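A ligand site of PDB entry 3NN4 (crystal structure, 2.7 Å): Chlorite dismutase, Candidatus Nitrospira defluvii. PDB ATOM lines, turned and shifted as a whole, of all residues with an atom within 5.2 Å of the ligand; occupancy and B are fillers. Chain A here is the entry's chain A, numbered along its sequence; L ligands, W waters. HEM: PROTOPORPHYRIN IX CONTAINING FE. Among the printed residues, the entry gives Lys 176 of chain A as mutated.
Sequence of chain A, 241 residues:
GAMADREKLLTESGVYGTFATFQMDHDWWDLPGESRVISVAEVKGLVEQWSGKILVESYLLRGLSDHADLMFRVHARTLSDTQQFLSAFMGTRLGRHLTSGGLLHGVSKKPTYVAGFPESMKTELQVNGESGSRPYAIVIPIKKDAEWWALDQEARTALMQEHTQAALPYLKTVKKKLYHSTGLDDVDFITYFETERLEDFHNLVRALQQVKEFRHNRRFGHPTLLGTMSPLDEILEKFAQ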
ATOM      1  N   LYS A 110       5.291  11.183  24.843  1.00  0.00           N
ATOM      2  CA  LYS A 110       5.180  12.094  23.693  1.00  0.00           C
ATOM      3  C   LYS A 110       6.556  12.763  23.445  1.00  0.00           C
ATOM      4  O   LYS A 110       7.293  13.023  24.418  1.00  0.00           O
ATOM      5  CB  LYS A 110       4.100  13.151  23.923  1.00  0.00           C
ATOM      6  CG  LYS A 110       2.781  12.588  24.470  1.00  0.00           C
ATOM      7  CD  LYS A 110       1.715  13.669  24.600  1.00  0.00           C
ATOM      8  CE  LYS A 110       0.503  13.169  25.374  1.00  0.00           C
ATOM      9  NZ  LYS A 110      -0.301  12.226  24.554  1.00  0.00           N
ATOM     10  N   PRO A 111       6.913  13.020  22.170  1.00  0.00           N
ATOM     11  CA  PRO A 111       8.321  13.366  21.842  1.00  0.00           C
ATOM     12  C   PRO A 111       8.761  14.767  22.339  1.00  0.00           C
ATOM     13  O   PRO A 111       8.019  15.745  22.172  1.00  0.00           O
ATOM     14  CB  PRO A 111       8.391  13.252  20.305  1.00  0.00           C
ATOM     15  CG  PRO A 111       7.018  12.706  19.864  1.00  0.00           C
ATOM     16  CD  PRO A 111       6.049  13.043  20.963  1.00  0.00           C
ATOM     17  N   THR A 112       9.958  14.819  22.934  1.00  0.00           N
ATOM     18  CA  THR A 112      10.507  16.018  23.609  1.00  0.00           C
ATOM     19  C   THR A 112      11.133  17.047  22.657  1.00  0.00           C
ATOM     20  O   THR A 112      11.013  18.259  22.870  1.00  0.00           O
ATOM     21  CB  THR A 112      11.570  15.615  24.699  1.00  0.00           C
ATOM     22  OG1 THR A 112      10.888  15.059  25.840  1.00  0.00           O
ATOM     23  CG2 THR A 112      12.455  16.823  25.128  1.00  0.00           C
ATOM     24  N   TYR A 113      11.817  16.574  21.610  1.00  0.00           N
ATOM     25  CA  TYR A 113      12.547  17.457  20.691  1.00  0.00           C
ATOM     26  C   TYR A 113      11.915  17.609  19.307  1.00  0.00           C
ATOM     27  O   TYR A 113      12.193  18.600  18.609  1.00  0.00           O
ATOM     28  CB  TYR A 113      13.974  16.947  20.535  1.00  0.00           C
ATOM     29  CG  TYR A 113      14.733  16.761  21.826  1.00  0.00           C
ATOM     30  CD1 TYR A 113      15.259  17.863  22.512  1.00  0.00           C
ATOM     31  CD2 TYR A 113      14.947  15.484  22.359  1.00  0.00           C
ATOM     32  CE1 TYR A 113      15.978  17.679  23.707  1.00  0.00           C
ATOM     33  CE2 TYR A 113      15.664  15.291  23.554  1.00  0.00           C
ATOM     34  CZ  TYR A 113      16.171  16.394  24.217  1.00  0.00           C
ATOM     35  OH  TYR A 113      16.864  16.204  25.381  1.00  0.00           O
ATOM     36  N   VAL A 114      11.067  16.659  18.896  1.00  0.00           N
ATOM     37  CA  VAL A 114      10.606  16.602  17.496  1.00  0.00           C
ATOM     38  C   VAL A 114       9.809  17.820  17.033  1.00  0.00           C
ATOM     39  O   VAL A 114       9.874  18.156  15.847  1.00  0.00           O
ATOM     40  CB  VAL A 114       9.807  15.315  17.172  1.00  0.00           C
ATOM     41  CG1 VAL A 114       9.065  15.445  15.836  1.00  0.00           C
ATOM     42  CG2 VAL A 114      10.744  14.115  17.136  1.00  0.00           C
ATOM     43  N   PHE A 117      12.068  20.434  15.444  1.00  0.00           N
ATOM     44  CA  PHE A 117      12.750  20.095  14.190  1.00  0.00           C
ATOM     45  C   PHE A 117      12.088  20.817  13.020  1.00  0.00           C
ATOM     46  O   PHE A 117      10.960  21.290  13.150  1.00  0.00           O
ATOM     47  CB  PHE A 117      12.703  18.581  13.907  1.00  0.00           C
ATOM     48  CG  PHE A 117      13.474  17.723  14.874  1.00  0.00           C
ATOM     49  CD1 PHE A 117      14.452  18.254  15.712  1.00  0.00           C
ATOM     50  CD2 PHE A 117      13.219  16.346  14.927  1.00  0.00           C
ATOM     51  CE1 PHE A 117      15.130  17.436  16.591  1.00  0.00           C
ATOM     52  CE2 PHE A 117      13.898  15.538  15.804  1.00  0.00           C
ATOM     53  CZ  PHE A 117      14.856  16.073  16.634  1.00  0.00           C
ATOM     54  N   LEU A 125       9.746  11.495   9.270  1.00  0.00           N
ATOM     55  CA  LEU A 125       9.542  10.707  10.518  1.00  0.00           C
ATOM     56  C   LEU A 125       8.161  10.042  10.602  1.00  0.00           C
ATOM     57  O   LEU A 125       7.997   9.022  11.270  1.00  0.00           O
ATOM     58  CB  LEU A 125       9.768  11.573  11.750  1.00  0.00           C
ATOM     59  CG  LEU A 125      11.230  11.926  12.026  1.00  0.00           C
ATOM     60  CD1 LEU A 125      11.337  13.056  13.054  1.00  0.00           C
ATOM     61  CD2 LEU A 125      11.970  10.667  12.493  1.00  0.00           C
ATOM     62  N   ILE A 140      18.597  -2.295  22.842  1.00  0.00           N
ATOM     63  CA  ILE A 140      19.799  -1.687  23.427  1.00  0.00           C
ATOM     64  C   ILE A 140      19.403  -0.710  24.516  1.00  0.00           C
ATOM     65  O   ILE A 140      18.827   0.318  24.205  1.00  0.00           O
ATOM     66  CB  ILE A 140      20.668  -0.932  22.372  1.00  0.00           C
ATOM     67  CG1 ILE A 140      21.107  -1.868  21.213  1.00  0.00           C
ATOM     68  CG2 ILE A 140      21.896  -0.346  23.024  1.00  0.00           C
ATOM     69  CD1 ILE A 140      21.231  -1.163  19.856  1.00  0.00           C
ATOM     70  N   ILE A 142      20.241   2.280  27.224  1.00  0.00           N
ATOM     71  CA  ILE A 142      21.105   3.415  27.043  1.00  0.00           C
ATOM     72  C   ILE A 142      21.073   4.291  28.279  1.00  0.00           C
ATOM     73  O   ILE A 142      19.997   4.552  28.853  1.00  0.00           O
ATOM     74  CB  ILE A 142      20.672   4.231  25.812  1.00  0.00           C
ATOM     75  CG1 ILE A 142      21.112   3.503  24.528  1.00  0.00           C
ATOM     76  CG2 ILE A 142      21.243   5.623  25.852  1.00  0.00           C
ATOM     77  CD1 ILE A 142      20.636   4.181  23.229  1.00  0.00           C
ATOM     78  N   LYS A 144      22.699   8.042  29.547  1.00  0.00           N
ATOM     79  CA  LYS A 144      23.359   9.280  29.128  1.00  0.00           C
ATOM     80  C   LYS A 144      24.351   9.728  30.193  1.00  0.00           C
ATOM     81  O   LYS A 144      24.229   9.307  31.329  1.00  0.00           O
ATOM     82  CB  LYS A 144      22.319  10.383  28.904  1.00  0.00           C
ATOM     83  CG  LYS A 144      21.447  10.194  27.672  1.00  0.00           C
ATOM     84  CD  LYS A 144      22.277  10.285  26.373  1.00  0.00           C
ATOM     85  CE  LYS A 144      21.377  10.485  25.146  1.00  0.00           C
ATOM     86  NZ  LYS A 144      22.121  10.570  23.838  1.00  0.00           N
ATOM     87  N   TRP A 148      25.351  15.379  29.275  1.00  0.00           N
ATOM     88  CA  TRP A 148      24.136  15.504  28.492  1.00  0.00           C
ATOM     89  C   TRP A 148      23.053  16.297  29.206  1.00  0.00           C
ATOM     90  O   TRP A 148      22.402  17.142  28.592  1.00  0.00           O
ATOM     91  CB  TRP A 148      23.589  14.126  28.161  1.00  0.00           C
ATOM     92  CG  TRP A 148      22.306  14.130  27.371  1.00  0.00           C
ATOM     93  CD1 TRP A 148      21.063  13.824  27.825  1.00  0.00           C
ATOM     94  CD2 TRP A 148      22.165  14.387  25.970  1.00  0.00           C
ATOM     95  NE1 TRP A 148      20.157  13.891  26.811  1.00  0.00           N
ATOM     96  CE2 TRP A 148      20.803  14.240  25.657  1.00  0.00           C
ATOM     97  CE3 TRP A 148      23.058  14.755  24.953  1.00  0.00           C
ATOM     98  CZ2 TRP A 148      20.298  14.447  24.367  1.00  0.00           C
ATOM     99  CZ3 TRP A 148      22.568  14.959  23.664  1.00  0.00           C
ATOM    100  CH2 TRP A 148      21.193  14.806  23.386  1.00  0.00           C
ATOM    101  N   MET A 160      19.857  16.144  18.917  1.00  0.00           N
ATOM    102  CA  MET A 160      18.851  15.160  18.528  1.00  0.00           C
ATOM    103  C   MET A 160      18.425  15.297  17.065  1.00  0.00           C
ATOM    104  O   MET A 160      18.112  14.307  16.436  1.00  0.00           O
ATOM    105  CB  MET A 160      17.639  15.243  19.454  1.00  0.00           C
ATOM    106  CG  MET A 160      17.885  14.686  20.860  1.00  0.00           C
ATOM    107  SD  MET A 160      18.933  13.187  20.851  1.00  0.00           S
ATOM    108  CE  MET A 160      17.962  12.089  19.817  1.00  0.00           C
ATOM    109  N   HIS A 163      21.004  13.526  15.195  1.00  0.00           N
ATOM    110  CA  HIS A 163      20.691  12.104  15.394  1.00  0.00           C
ATOM    111  C   HIS A 163      19.654  11.635  14.390  1.00  0.00           C
ATOM    112  O   HIS A 163      19.895  10.676  13.648  1.00  0.00           O
ATOM    113  CB  HIS A 163      20.173  11.899  16.843  1.00  0.00           C
ATOM    114  CG  HIS A 163      19.570  10.555  17.117  1.00  0.00           C
ATOM    115  ND1 HIS A 163      20.293   9.388  17.052  1.00  0.00           N
ATOM    116  CD2 HIS A 163      18.328  10.206  17.503  1.00  0.00           C
ATOM    117  CE1 HIS A 163      19.498   8.368  17.353  1.00  0.00           C
ATOM    118  NE2 HIS A 163      18.296   8.849  17.647  1.00  0.00           N
ATOM    119  N   THR A 164      18.512  12.336  14.357  1.00  0.00           N
ATOM    120  CA  THR A 164      17.393  11.998  13.494  1.00  0.00           C
ATOM    121  C   THR A 164      17.762  12.052  12.011  1.00  0.00           C
ATOM    122  O   THR A 164      17.362  11.200  11.231  1.00  0.00           O
ATOM    123  CB  THR A 164      16.182  12.924  13.755  1.00  0.00           C
ATOM    124  OG1 THR A 164      15.633  12.637  15.042  1.00  0.00           O
ATOM    125  CG2 THR A 164      15.102  12.714  12.704  1.00  0.00           C
ATOM    126  N   ALA A 167      19.735   9.037  10.865  1.00  0.00           N
ATOM    127  CA  ALA A 167      18.978   7.790  10.948  1.00  0.00           C
ATOM    128  C   ALA A 167      17.784   7.662  10.010  1.00  0.00           C
ATOM    129  O   ALA A 167      17.287   6.556   9.804  1.00  0.00           O
ATOM    130  CB  ALA A 167      18.490   7.580  12.386  1.00  0.00           C
ATOM    131  N   LEU A 168      17.287   8.770   9.474  1.00  0.00           N
ATOM    132  CA  LEU A 168      16.074   8.752   8.663  1.00  0.00           C
ATOM    133  C   LEU A 168      16.111   7.766   7.491  1.00  0.00           C
ATOM    134  O   LEU A 168      15.176   6.982   7.333  1.00  0.00           O
ATOM    135  CB  LEU A 168      15.726  10.151   8.147  1.00  0.00           C
ATOM    136  CG  LEU A 168      14.789  10.980   9.029  1.00  0.00           C
ATOM    137  CD1 LEU A 168      14.804  12.440   8.636  1.00  0.00           C
ATOM    138  CD2 LEU A 168      13.375  10.416   8.955  1.00  0.00           C
ATOM    139  N   TYR A 170      17.214   4.988   7.110  1.00  0.00           N
ATOM    140  CA  TYR A 170      17.013   3.620   7.559  1.00  0.00           C
ATOM    141  C   TYR A 170      15.594   3.333   8.081  1.00  0.00           C
ATOM    142  O   TYR A 170      15.268   2.191   8.391  1.00  0.00           O
ATOM    143  CB  TYR A 170      18.063   3.258   8.625  1.00  0.00           C
ATOM    144  CG  TYR A 170      19.477   3.312   8.101  1.00  0.00           C
ATOM    145  CD1 TYR A 170      20.000   2.240   7.392  1.00  0.00           C
ATOM    146  CD2 TYR A 170      20.274   4.442   8.284  1.00  0.00           C
ATOM    147  CE1 TYR A 170      21.302   2.282   6.880  1.00  0.00           C
ATOM    148  CE2 TYR A 170      21.577   4.484   7.772  1.00  0.00           C
ATOM    149  CZ  TYR A 170      22.081   3.395   7.077  1.00  0.00           C
ATOM    150  OH  TYR A 170      23.333   3.383   6.563  1.00  0.00           O
ATOM    151  N   LEU A 171      14.747   4.370   8.185  1.00  0.00           N
ATOM    152  CA  LEU A 171      13.338   4.158   8.575  1.00  0.00           C
ATOM    153  C   LEU A 171      12.591   3.250   7.595  1.00  0.00           C
ATOM    154  O   LEU A 171      11.619   2.596   7.980  1.00  0.00           O
ATOM    155  CB  LEU A 171      12.567   5.488   8.720  1.00  0.00           C
ATOM    156  CG  LEU A 171      12.427   6.173  10.091  1.00  0.00           C
ATOM    157  CD1 LEU A 171      11.539   7.388   9.946  1.00  0.00           C
ATOM    158  CD2 LEU A 171      11.868   5.251  11.178  1.00  0.00           C
ATOM    159  N   VAL A 174      13.892  -0.350   8.907  1.00  0.00           N
ATOM    160  CA  VAL A 174      14.024  -0.584  10.356  1.00  0.00           C
ATOM    161  C   VAL A 174      12.902   0.108  11.157  1.00  0.00           C
ATOM    162  O   VAL A 174      12.755   1.333  11.096  1.00  0.00           O
ATOM    163  CB  VAL A 174      15.402  -0.086  10.892  1.00  0.00           C
ATOM    164  CG1 VAL A 174      15.448  -0.172  12.410  1.00  0.00           C
ATOM    165  CG2 VAL A 174      16.546  -0.875  10.283  1.00  0.00           C
ATOM    166  N   LYS A 176      11.177   1.117  14.928  1.00  0.00           N
ATOM    167  CA  LYS A 176      11.819   1.595  16.164  1.00  0.00           C
ATOM    168  C   LYS A 176      10.778   1.912  17.243  1.00  0.00           C
ATOM    169  O   LYS A 176       9.648   2.226  16.948  1.00  0.00           O
ATOM    170  CB  LYS A 176      12.696   2.825  15.866  1.00  0.00           C
ATOM    171  CG  LYS A 176      11.977   4.152  16.122  1.00  0.00           C
ATOM    172  CD  LYS A 176      12.556   5.327  15.350  1.00  0.00           C
ATOM    173  CE  LYS A 176      11.835   6.650  15.763  1.00  0.00           C
ATOM    174  NZ  LYS A 176      12.027   6.985  17.249  1.00  0.00           N
ATOM    175  N   LEU A 178      10.835   3.747  21.457  1.00  0.00           N
ATOM    176  CA  LEU A 178      11.654   4.322  22.506  1.00  0.00           C
ATOM    177  C   LEU A 178      10.851   4.307  23.789  1.00  0.00           C
ATOM    178  O   LEU A 178       9.695   4.698  23.793  1.00  0.00           O
ATOM    179  CB  LEU A 178      12.074   5.750  22.117  1.00  0.00           C
ATOM    180  CG  LEU A 178      12.948   6.488  23.148  1.00  0.00           C
ATOM    181  CD1 LEU A 178      14.349   5.889  23.186  1.00  0.00           C
ATOM    182  CD2 LEU A 178      12.963   7.994  22.887  1.00  0.00           C
ATOM    183  N   HIS A 180      10.900   5.432  27.950  1.00  0.00           N
ATOM    184  CA  HIS A 180      11.572   6.299  28.897  1.00  0.00           C
ATOM    185  C   HIS A 180      11.722   5.603  30.266  1.00  0.00           C
ATOM    186  O   HIS A 180      10.744   5.408  30.967  1.00  0.00           O
ATOM    187  CB  HIS A 180      10.870   7.634  28.934  1.00  0.00           C
ATOM    188  CG  HIS A 180      10.877   8.338  27.593  1.00  0.00           C
ATOM    189  ND1 HIS A 180      11.659   9.442  27.335  1.00  0.00           N
ATOM    190  CD2 HIS A 180      10.181   8.095  26.460  1.00  0.00           C
ATOM    191  CE1 HIS A 180      11.439   9.861  26.103  1.00  0.00           C
ATOM    192  NE2 HIS A 180      10.549   9.053  25.545  1.00  0.00           N
ATOM    193  N   PHE A 189      16.992   5.098  28.886  1.00  0.00           N
ATOM    194  CA  PHE A 189      16.089   4.707  27.805  1.00  0.00           C
ATOM    195  C   PHE A 189      16.260   3.239  27.491  1.00  0.00           C
ATOM    196  O   PHE A 189      17.316   2.641  27.745  1.00  0.00           O
ATOM    197  CB  PHE A 189      16.329   5.539  26.544  1.00  0.00           C
ATOM    198  CG  PHE A 189      16.404   7.016  26.789  1.00  0.00           C
ATOM    199  CD1 PHE A 189      15.248   7.758  26.951  1.00  0.00           C
ATOM    200  CD2 PHE A 189      17.605   7.655  26.874  1.00  0.00           C
ATOM    201  CE1 PHE A 189      15.308   9.125  27.172  1.00  0.00           C
ATOM    202  CE2 PHE A 189      17.681   9.000  27.119  1.00  0.00           C
ATOM    203  CZ  PHE A 189      16.525   9.742  27.281  1.00  0.00           C
ATOM    204  N   THR A 191      15.819   1.177  23.958  1.00  0.00           N
ATOM    205  CA  THR A 191      15.553   1.240  22.513  1.00  0.00           C
ATOM    206  C   THR A 191      15.223  -0.179  21.978  1.00  0.00           C
ATOM    207  O   THR A 191      15.814  -1.175  22.395  1.00  0.00           O
ATOM    208  CB  THR A 191      16.719   1.909  21.726  1.00  0.00           C
ATOM    209  OG1 THR A 191      17.921   1.141  21.847  1.00  0.00           O
ATOM    210  CG2 THR A 191      16.980   3.327  22.240  1.00  0.00           C
ATOM    211  N   PHE A 193      13.966  -2.405  18.305  1.00  0.00           N
ATOM    212  CA  PHE A 193      13.961  -2.343  16.843  1.00  0.00           C
ATOM    213  C   PHE A 193      13.535  -3.650  16.214  1.00  0.00           C
ATOM    214  O   PHE A 193      13.850  -4.700  16.722  1.00  0.00           O
ATOM    215  CB  PHE A 193      15.348  -2.031  16.324  1.00  0.00           C
ATOM    216  CG  PHE A 193      15.945  -0.813  16.910  1.00  0.00           C
ATOM    217  CD1 PHE A 193      16.674  -0.898  18.079  1.00  0.00           C
ATOM    218  CD2 PHE A 193      15.803   0.409  16.302  1.00  0.00           C
ATOM    219  CE1 PHE A 193      17.236   0.213  18.632  1.00  0.00           C
ATOM    220  CE2 PHE A 193      16.374   1.539  16.862  1.00  0.00           C
ATOM    221  CZ  PHE A 193      17.094   1.435  18.024  1.00  0.00           C
ATOM    222  N   PHE A 201      20.651  -2.541   9.805  1.00  0.00           N
ATOM    223  CA  PHE A 201      20.661  -2.130  11.212  1.00  0.00           C
ATOM    224  C   PHE A 201      22.072  -1.813  11.656  1.00  0.00           C
ATOM    225  O   PHE A 201      22.313  -0.858  12.379  1.00  0.00           O
ATOM    226  CB  PHE A 201      20.034  -3.191  12.123  1.00  0.00           C
ATOM    227  CG  PHE A 201      19.964  -2.766  13.558  1.00  0.00           C
ATOM    228  CD1 PHE A 201      19.003  -1.852  13.964  1.00  0.00           C
ATOM    229  CD2 PHE A 201      20.885  -3.225  14.489  1.00  0.00           C
ATOM    230  CE1 PHE A 201      18.947  -1.425  15.272  1.00  0.00           C
ATOM    231  CE2 PHE A 201      20.844  -2.790  15.798  1.00  0.00           C
ATOM    232  CZ  PHE A 201      19.867  -1.894  16.189  1.00  0.00           C
ATOM    233  N   LEU A 204      22.957   1.489  10.310  1.00  0.00           N
ATOM    234  CA  LEU A 204      22.227   2.514  11.080  1.00  0.00           C
ATOM    235  C   LEU A 204      23.006   2.882  12.350  1.00  0.00           C
ATOM    236  O   LEU A 204      23.277   4.056  12.616  1.00  0.00           O
ATOM    237  CB  LEU A 204      20.822   2.006  11.417  1.00  0.00           C
ATOM    238  CG  LEU A 204      20.031   2.750  12.510  1.00  0.00           C
ATOM    239  CD1 LEU A 204      19.877   4.239  12.192  1.00  0.00           C
ATOM    240  CD2 LEU A 204      18.681   2.115  12.688  1.00  0.00           C
ATOM    241  N   VAL A 205      23.370   1.865  13.131  1.00  0.00           N
ATOM    242  CA  VAL A 205      24.178   2.084  14.327  1.00  0.00           C
ATOM    243  C   VAL A 205      25.541   2.711  14.008  1.00  0.00           C
ATOM    244  O   VAL A 205      26.019   3.550  14.775  1.00  0.00           O
ATOM    245  CB  VAL A 205      24.437   0.760  15.115  1.00  0.00           C
ATOM    246  CG1 VAL A 205      25.361   1.031  16.311  1.00  0.00           C
ATOM    247  CG2 VAL A 205      23.118   0.142  15.579  1.00  0.00           C
ATOM    248  N   LEU A 208      25.037   6.417  13.348  1.00  0.00           N
ATOM    249  CA  LEU A 208      24.796   7.114  14.610  1.00  0.00           C
ATOM    250  C   LEU A 208      26.023   7.315  15.476  1.00  0.00           C
ATOM    251  O   LEU A 208      26.092   8.287  16.225  1.00  0.00           O
ATOM    252  CB  LEU A 208      23.746   6.378  15.426  1.00  0.00           C
ATOM    253  CG  LEU A 208      22.357   6.465  14.806  1.00  0.00           C
ATOM    254  CD1 LEU A 208      21.516   5.351  15.344  1.00  0.00           C
ATOM    255  CD2 LEU A 208      21.751   7.836  15.078  1.00  0.00           C
ATOM    256  N   GLU A 213      26.076  13.553  19.380  1.00  0.00           N
ATOM    257  CA  GLU A 213      25.258  13.036  20.491  1.00  0.00           C
ATOM    258  C   GLU A 213      25.785  11.712  21.049  1.00  0.00           C
ATOM    259  O   GLU A 213      25.608  11.455  22.255  1.00  0.00           O
ATOM    260  CB  GLU A 213      23.793  12.879  20.041  1.00  0.00           C
ATOM    261  CG  GLU A 213      22.825  12.189  21.040  1.00  0.00           C
ATOM    262  CD  GLU A 213      22.328  10.848  20.556  1.00  0.00           C
ATOM    263  OE1 GLU A 213      22.887  10.336  19.556  1.00  0.00           O
ATOM    264  OE2 GLU A 213      21.376  10.292  21.180  1.00  0.00           O
ATOM    265  N   PHE A 220      26.055   2.061  26.485  1.00  0.00           N
ATOM    266  CA  PHE A 220      25.490   1.710  25.185  1.00  0.00           C
ATOM    267  C   PHE A 220      25.531   0.198  25.024  1.00  0.00           C
ATOM    268  O   PHE A 220      26.545  -0.381  24.590  1.00  0.00           O
ATOM    269  CB  PHE A 220      26.257   2.406  24.052  1.00  0.00           C
ATOM    270  CG  PHE A 220      25.511   2.438  22.763  1.00  0.00           C
ATOM    271  CD1 PHE A 220      24.439   3.315  22.584  1.00  0.00           C
ATOM    272  CD2 PHE A 220      25.845   1.575  21.747  1.00  0.00           C
ATOM    273  CE1 PHE A 220      23.739   3.333  21.386  1.00  0.00           C
ATOM    274  CE2 PHE A 220      25.151   1.592  20.557  1.00  0.00           C
ATOM    275  CZ  PHE A 220      24.099   2.456  20.374  1.00  0.00           C
HETATM  276  CHA HEM L   1      15.508   9.760  20.220  1.00  0.00           C
HETATM  277  CHB HEM L   1      14.551   9.077  15.544  1.00  0.00           C
HETATM  278  CHC HEM L   1      17.422   5.155  15.657  1.00  0.00           C
HETATM  279  CHD HEM L   1      18.550   5.931  20.280  1.00  0.00           C
HETATM  280  C1A HEM L   1      15.005   9.948  18.967  1.00  0.00           C
HETATM  281  C2A HEM L   1      14.148  11.035  18.540  1.00  0.00           C
HETATM  282  C3A HEM L   1      13.903  10.857  17.240  1.00  0.00           C
HETATM  283  C4A HEM L   1      14.570   9.643  16.816  1.00  0.00           C
HETATM  284  CMA HEM L   1      13.028  11.724  16.319  1.00  0.00           C
HETATM  285  CAA HEM L   1      13.652  12.211  19.417  1.00  0.00           C
HETATM  286  CBA HEM L   1      12.506  11.829  20.354  1.00  0.00           C
HETATM  287  CGA HEM L   1      12.008  13.080  21.083  1.00  0.00           C
HETATM  288  O1A HEM L   1      11.592  14.069  20.420  1.00  0.00           O
HETATM  289  O2A HEM L   1      11.979  13.137  22.351  1.00  0.00           O
HETATM  290  C1B HEM L   1      15.212   7.917  15.180  1.00  0.00           C
HETATM  291  C2B HEM L   1      15.097   7.235  13.912  1.00  0.00           C
HETATM  292  C3B HEM L   1      15.884   6.183  13.946  1.00  0.00           C
HETATM  293  C4B HEM L   1      16.532   6.127  15.248  1.00  0.00           C
HETATM  294  CMB HEM L   1      14.240   7.631  12.692  1.00  0.00           C
HETATM  295  CAB HEM L   1      16.044   5.199  12.778  1.00  0.00           C
HETATM  296  CBB HEM L   1      15.359   4.050  12.799  1.00  0.00           C
HETATM  297  C1C HEM L   1      18.011   5.045  16.900  1.00  0.00           C
HETATM  298  C2C HEM L   1      19.015   4.085  17.269  1.00  0.00           C
HETATM  299  C3C HEM L   1      19.318   4.304  18.552  1.00  0.00           C
HETATM  300  C4C HEM L   1      18.527   5.397  19.028  1.00  0.00           C
HETATM  301  CMC HEM L   1      19.615   2.992  16.341  1.00  0.00           C
HETATM  302  CAC HEM L   1      20.344   3.532  19.396  1.00  0.00           C
HETATM  303  CBC HEM L   1      20.581   2.238  19.121  1.00  0.00           C
HETATM  304  C1D HEM L   1      17.810   6.995  20.713  1.00  0.00           C
HETATM  305  C2D HEM L   1      17.733   7.468  22.081  1.00  0.00           C
HETATM  306  C3D HEM L   1      16.795   8.654  22.025  1.00  0.00           C
HETATM  307  C4D HEM L   1      16.395   8.781  20.657  1.00  0.00           C
HETATM  308  CMD HEM L   1      18.444   6.944  23.344  1.00  0.00           C
HETATM  309  CAD HEM L   1      16.374   9.527  23.203  1.00  0.00           C
HETATM  310  CBD HEM L   1      16.958  10.930  23.066  1.00  0.00           C
HETATM  311  CGD HEM L   1      18.415  10.892  23.441  1.00  0.00           C
HETATM  312  O1D HEM L   1      18.721  11.328  24.598  1.00  0.00           O
HETATM  313  O2D HEM L   1      19.250  10.415  22.594  1.00  0.00           O
HETATM  314  NA  HEM L   1      15.241   9.119  17.904  1.00  0.00           N
HETATM  315  NB  HEM L   1      16.093   7.207  15.993  1.00  0.00           N
HETATM  316  NC  HEM L   1      17.728   5.832  17.996  1.00  0.00           N
HETATM  317  ND  HEM L   1      17.000   7.795  19.902  1.00  0.00           N
HETATM  318 FE   HEM L   1      16.596   7.552  17.885  1.00  0.00          FE
HETATM  319  O   HOH W   1      14.411   6.029  18.460  1.00  0.00           O
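An oxygen (O2D) of the ligand sits close to the side-chain sulfur of Met 160 (3.3 Å). Pro 111 touches the ligand. CE2 of Phe 117 touches CMA of the ligand (3.9 Å). CD2 of Leu 125 touches CMB of the ligand (3.8 Å). CD1 of Ile 140 touches CBC of the ligand, at 3.5 Å. Ile 142 touches the ligand. Trp 148 touches the ligand. Thr 164 touches the ligand (OG1 to CMA, 3.0 Å). Ala 167 touches the ligand (CB to C3B, 3.3 Å). Leu 171 touches the ligand (CG to CMB, 3.5 Å). Lys 176 touches the ligand (CD to C2B, 3.5 Å). CD2 of Leu 178 touches CAD of the ligand (3.8 Å). CE2 of Phe 189 touches O1D of the ligand (3.6 Å). Thr 191 touches the ligand. CZ of Phe 193 touches C2C of the ligand (3.4 Å). CD2 of Leu 204 touches CBB of the ligand, at 3.8 Å. CD1 of Leu 208 touches CMC of the ligand, at 3.2 Å. CZ of Phe 220 touches CBC of the ligand, 3.7 Å away. Within 4 Å of the ligand: Pro 111, Thr 112, Tyr 113, Val 114, Phe 117, Leu 125, Ile 140, Ile 142, Lys 144, Trp 148, Met 160, His 163, Thr 164, Ala 167, Leu 171, Lys 176, Leu 178, Phe 189, Thr 191, Phe 193, Leu 204, Leu 208, Glu 213 and Phe 220.
NE2 of His 163 binds FE of the ligand (2.2 Å). An oxygen (O2D) of the ligand lies close to the side-chain carboxylate (OE2) of Glu 213. The backbone NH of Thr 112 is in hydrogen-bond range of an oxygen (O2A) of the ligand (2.7 Å). O1A of the ligand is in hydrogen-bond range of N of Tyr 113 (2.8 Å). The side-chain amino group (NZ) of Lys 144 lies within salt-bridge range of an oxygen (O2D) of the ligand. O1A of the ligand sits at hydrogen-bond distance from N of Val 114 (3.1 Å).
The side-chain carboxylate of Glu 213 lies within salt-bridge range of the side-chain amino group of Lys 144, at 2.8 Å. O of Met 160 lies within hydrogen-bond range of OG1 of Thr 164 (3.3 Å). O of Phe 189 lies within hydrogen-bond range of N of Ile 142. The backbone carbonyl oxygen (O) of Ile 140 is in hydrogen-bond range of the side-chain hydroxyl (OG1) of Thr 191, 2.7 Å away.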
